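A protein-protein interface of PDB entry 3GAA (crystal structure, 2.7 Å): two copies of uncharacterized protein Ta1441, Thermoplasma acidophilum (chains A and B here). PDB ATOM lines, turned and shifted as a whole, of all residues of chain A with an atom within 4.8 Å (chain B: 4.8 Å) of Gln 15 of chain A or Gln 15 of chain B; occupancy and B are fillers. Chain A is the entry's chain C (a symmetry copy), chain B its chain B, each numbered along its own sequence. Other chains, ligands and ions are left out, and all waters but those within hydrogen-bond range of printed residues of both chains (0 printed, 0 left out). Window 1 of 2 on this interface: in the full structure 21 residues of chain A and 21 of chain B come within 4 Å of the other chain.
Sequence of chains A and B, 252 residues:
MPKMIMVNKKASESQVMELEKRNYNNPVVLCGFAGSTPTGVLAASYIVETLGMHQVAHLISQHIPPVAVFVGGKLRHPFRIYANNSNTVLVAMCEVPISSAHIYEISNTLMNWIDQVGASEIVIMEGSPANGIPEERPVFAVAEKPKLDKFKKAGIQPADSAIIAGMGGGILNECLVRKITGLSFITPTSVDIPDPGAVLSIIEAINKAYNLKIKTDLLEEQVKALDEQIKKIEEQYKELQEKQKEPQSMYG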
ATOM      1  N   SER A  12      21.292  23.868  21.015  1.00  0.00           N
ATOM      2  CA  SER A  12      21.468  23.727  19.588  1.00  0.00           C
ATOM      3  C   SER A  12      22.005  22.367  19.194  1.00  0.00           C
ATOM      4  O   SER A  12      22.138  22.063  18.037  1.00  0.00           O
ATOM      5  CB  SER A  12      22.318  24.850  19.039  1.00  0.00           C
ATOM      6  OG  SER A  12      23.579  24.817  19.620  1.00  0.00           O
ATOM      7  N   GLU A  13      22.286  21.530  20.165  1.00  0.00           N
ATOM      8  CA  GLU A  13      22.590  20.110  19.846  1.00  0.00           C
ATOM      9  C   GLU A  13      21.679  19.410  18.792  1.00  0.00           C
ATOM     10  O   GLU A  13      22.179  18.722  17.913  1.00  0.00           O
ATOM     11  CB  GLU A  13      22.590  19.272  21.117  1.00  0.00           C
ATOM     12  CG  GLU A  13      21.952  19.972  22.341  1.00  0.00           C
ATOM     13  CD  GLU A  13      22.990  20.655  23.190  1.00  0.00           C
ATOM     14  OE1 GLU A  13      22.650  21.341  24.171  1.00  0.00           O
ATOM     15  OE2 GLU A  13      24.190  20.448  22.912  1.00  0.00           O
ATOM     16  N   SER A  14      20.352  19.545  18.885  1.00  0.00           N
ATOM     17  CA  SER A  14      19.425  18.979  17.850  1.00  0.00           C
ATOM     18  C   SER A  14      19.956  19.257  16.443  1.00  0.00           C
ATOM     19  O   SER A  14      20.049  18.392  15.556  1.00  0.00           O
ATOM     20  CB  SER A  14      18.029  19.609  17.995  1.00  0.00           C
ATOM     21  OG  SER A  14      18.094  20.907  18.588  1.00  0.00           O
ATOM     22  N   GLN A  15      20.310  20.522  16.295  1.00  0.00           N
ATOM     23  CA  GLN A  15      20.886  21.091  15.111  1.00  0.00           C
ATOM     24  C   GLN A  15      22.295  20.583  14.812  1.00  0.00           C
ATOM     25  O   GLN A  15      22.420  19.912  13.794  1.00  0.00           O
ATOM     26  CB  GLN A  15      20.915  22.606  15.320  1.00  0.00           C
ATOM     27  CG  GLN A  15      20.054  23.411  14.432  1.00  0.00           C
ATOM     28  CD  GLN A  15      20.542  23.292  13.048  1.00  0.00           C
ATOM     29  OE1 GLN A  15      20.565  22.189  12.504  1.00  0.00           O
ATOM     30  NE2 GLN A  15      20.998  24.425  12.466  1.00  0.00           N
ATOM     31  N   VAL A  16      23.326  20.850  15.678  1.00  0.00           N
ATOM     32  CA  VAL A  16      24.736  20.533  15.314  1.00  0.00           C
ATOM     33  C   VAL A  16      24.816  19.071  14.993  1.00  0.00           C
ATOM     34  O   VAL A  16      25.573  18.688  14.115  1.00  0.00           O
ATOM     35  CB  VAL A  16      25.923  20.971  16.336  1.00  0.00           C
ATOM     36  CG1 VAL A  16      26.926  19.861  16.653  1.00  0.00           C
ATOM     37  CG2 VAL A  16      26.782  22.086  15.739  1.00  0.00           C
ATOM     38  N   MET A  17      24.007  18.259  15.658  1.00  0.00           N
ATOM     39  CA  MET A  17      24.195  16.821  15.642  1.00  0.00           C
ATOM     40  C   MET A  17      23.143  16.012  14.836  1.00  0.00           C
ATOM     41  O   MET A  17      23.337  14.809  14.649  1.00  0.00           O
ATOM     42  CB  MET A  17      24.342  16.334  17.095  1.00  0.00           C
ATOM     43  CG  MET A  17      25.718  15.879  17.428  1.00  0.00           C
ATOM     44  SD  MET A  17      26.915  16.928  18.325  1.00  0.00           S
ATOM     45  CE  MET A  17      28.423  16.182  17.698  1.00  0.00           C
ATOM     46  N   GLU A  18      22.097  16.676  14.301  1.00  0.00           N
ATOM     47  CA  GLU A  18      20.924  16.012  13.704  1.00  0.00           C
ATOM     48  C   GLU A  18      20.372  14.936  14.644  1.00  0.00           C
ATOM     49  O   GLU A  18      20.538  13.738  14.402  1.00  0.00           O
ATOM     50  CB  GLU A  18      21.276  15.348  12.396  1.00  0.00           C
ATOM     51  CG  GLU A  18      22.392  15.992  11.603  1.00  0.00           C
ATOM     52  CD  GLU A  18      21.966  17.187  10.743  1.00  0.00           C
ATOM     53  OE1 GLU A  18      22.482  17.217   9.604  1.00  0.00           O
ATOM     54  OE2 GLU A  18      21.160  18.069  11.173  1.00  0.00           O
ATOM     55  N   GLU A  20      17.138  15.086  16.359  1.00  0.00           N
ATOM     56  CA  GLU A  20      15.835  15.651  16.694  1.00  0.00           C
ATOM     57  C   GLU A  20      14.932  14.713  17.482  1.00  0.00           C
ATOM     58  O   GLU A  20      14.293  15.144  18.428  1.00  0.00           O
ATOM     59  CB  GLU A  20      15.104  16.084  15.427  1.00  0.00           C
ATOM     60  CG  GLU A  20      14.369  17.396  15.592  1.00  0.00           C
ATOM     61  CD  GLU A  20      15.311  18.436  16.121  1.00  0.00           C
ATOM     62  OE1 GLU A  20      15.230  18.694  17.351  1.00  0.00           O
ATOM     63  OE2 GLU A  20      16.169  18.924  15.325  1.00  0.00           O
ATOM     64  N   SER B  12      17.104  27.032  17.391  1.00  0.00           N
ATOM     65  CA  SER B  12      18.359  26.942  16.702  1.00  0.00           C
ATOM     66  C   SER B  12      18.558  28.078  15.756  1.00  0.00           C
ATOM     67  O   SER B  12      19.559  28.149  15.094  1.00  0.00           O
ATOM     68  CB  SER B  12      18.452  25.643  15.952  1.00  0.00           C
ATOM     69  OG  SER B  12      17.172  25.193  15.661  1.00  0.00           O
ATOM     70  N   GLU B  13      17.628  28.998  15.683  1.00  0.00           N
ATOM     71  CA  GLU B  13      17.896  30.141  14.759  1.00  0.00           C
ATOM     72  C   GLU B  13      19.363  30.626  14.741  1.00  0.00           C
ATOM     73  O   GLU B  13      19.979  30.721  13.693  1.00  0.00           O
ATOM     74  CB  GLU B  13      16.984  31.350  15.006  1.00  0.00           C
ATOM     75  CG  GLU B  13      16.376  31.432  16.405  1.00  0.00           C
ATOM     76  CD  GLU B  13      14.964  30.815  16.488  1.00  0.00           C
ATOM     77  OE1 GLU B  13      14.257  31.107  17.483  1.00  0.00           O
ATOM     78  OE2 GLU B  13      14.554  30.056  15.574  1.00  0.00           O
ATOM     79  N   SER B  14      19.913  30.924  15.910  1.00  0.00           N
ATOM     80  CA  SER B  14      21.216  31.580  15.993  1.00  0.00           C
ATOM     81  C   SER B  14      22.343  30.664  15.457  1.00  0.00           C
ATOM     82  O   SER B  14      23.459  31.086  15.152  1.00  0.00           O
ATOM     83  CB  SER B  14      21.430  32.106  17.429  1.00  0.00           C
ATOM     84  OG  SER B  14      20.455  33.145  17.745  1.00  0.00           O
ATOM     85  N   GLN B  15      21.971  29.413  15.261  1.00  0.00           N
ATOM     86  CA  GLN B  15      22.771  28.399  14.600  1.00  0.00           C
ATOM     87  C   GLN B  15      22.567  28.251  13.062  1.00  0.00           C
ATOM     88  O   GLN B  15      23.550  28.364  12.344  1.00  0.00           O
ATOM     89  CB  GLN B  15      22.428  27.093  15.278  1.00  0.00           C
ATOM     90  CG  GLN B  15      23.544  26.437  15.924  1.00  0.00           C
ATOM     91  CD  GLN B  15      24.238  25.607  14.924  1.00  0.00           C
ATOM     92  OE1 GLN B  15      25.174  26.069  14.252  1.00  0.00           O
ATOM     93  NE2 GLN B  15      23.744  24.374  14.748  1.00  0.00           N
ATOM     94  N   VAL B  16      21.332  28.004  12.552  1.00  0.00           N
ATOM     95  CA  VAL B  16      21.094  27.981  11.077  1.00  0.00           C
ATOM     96  C   VAL B  16      21.663  29.267  10.522  1.00  0.00           C
ATOM     97  O   VAL B  16      22.448  29.227   9.602  1.00  0.00           O
ATOM     98  CB  VAL B  16      19.560  27.754  10.564  1.00  0.00           C
ATOM     99  CG1 VAL B  16      19.190  28.627   9.343  1.00  0.00           C
ATOM    100  CG2 VAL B  16      19.295  26.299  10.149  1.00  0.00           C
ATOM    101  N   MET B  17      21.334  30.397  11.140  1.00  0.00           N
ATOM    102  CA  MET B  17      21.588  31.707  10.540  1.00  0.00           C
ATOM    103  C   MET B  17      22.961  32.273  10.939  1.00  0.00           C
ATOM    104  O   MET B  17      23.279  33.403  10.541  1.00  0.00           O
ATOM    105  CB  MET B  17      20.458  32.732  10.877  1.00  0.00           C
ATOM    106  CG  MET B  17      19.003  32.188  11.043  1.00  0.00           C
ATOM    107  SD  MET B  17      18.040  31.999   9.514  1.00  0.00           S
ATOM    108  CE  MET B  17      19.299  31.803   8.255  1.00  0.00           C
ATOM    109  N   GLU B  18      23.775  31.490  11.669  1.00  0.00           N
ATOM    110  CA  GLU B  18      25.002  31.988  12.352  1.00  0.00           C
ATOM    111  C   GLU B  18      24.860  33.439  12.878  1.00  0.00           C
ATOM    112  O   GLU B  18      25.550  34.352  12.443  1.00  0.00           O
ATOM    113  CB  GLU B  18      26.292  31.778  11.515  1.00  0.00           C
ATOM    114  CG  GLU B  18      26.253  32.143  10.000  1.00  0.00           C
ATOM    115  CD  GLU B  18      26.256  30.901   9.010  1.00  0.00           C
ATOM    116  OE1 GLU B  18      25.660  30.966   7.880  1.00  0.00           O
ATOM    117  OE2 GLU B  18      26.872  29.870   9.373  1.00  0.00           O
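Ser 12 of chain A touches Gln 15 of chain B, and with the chains exchanged Gln 15 of chain A touches Ser 12 of chain B. Gln 15 of chain B touches its own counterpart, Gln 15 of chain A. Gln 15 of chain A touches Val 16 of chain B, and with the chains exchanged Val 16 of chain A touches Gln 15 of chain B. Positions printed for both chains: 12, 13, 14, 15, 16, 17 and 18.
CG of Gln 15 of chain B touches CB of Ser 12 of chain A, 3.7 Å away. Ser 12 of chain B touches Gln 15 of chain A (CB to CG, 3.1 Å). Gln 15 of chain A touches Gln 15 of chain B. CG2 of Val 16 of chain B touches NE2 of Gln 15 of chain A, at 3.4 Å. Gln 15 of chain B touches Val 16 of chain A (NE2 to N, 3.7 Å).
Of the 7 printed residues of chain B, 3 touch a printed residue of chain A. Hydrophobic or aromatic side chains of chain B that line the printed part of chain A: Val 16. Along chain B the printed residues that touch a printed residue of chain A span positions 12 to 16. Hydrophobic or aromatic side chains of chain A that line the printed part of chain B: Val 16. Among the printed residues, 5 pairs touch across the chains. Among the printed residues, no Asp or Glu carboxylate lies within 4 Å of a Lys or Arg side-chain nitrogen of the other chain.
Printed residues of chain B within 4 Å of Ser 12 of chain A: Gln 15. Of chain B, only Ser 12 (3.1 Å), Gln 15 (3.4 Å) and Val 16 (3.4 Å) come within 4 Å of Gln 15 of chain A. Printed residues of chain B within 4 Å of Val 16 of chain A: Gln 15. Of the printed residues of chain A, Ser 12 of chain B touches Gln 15. Of the printed residues of chain A, Val 16 of chain B touches Gln 15.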
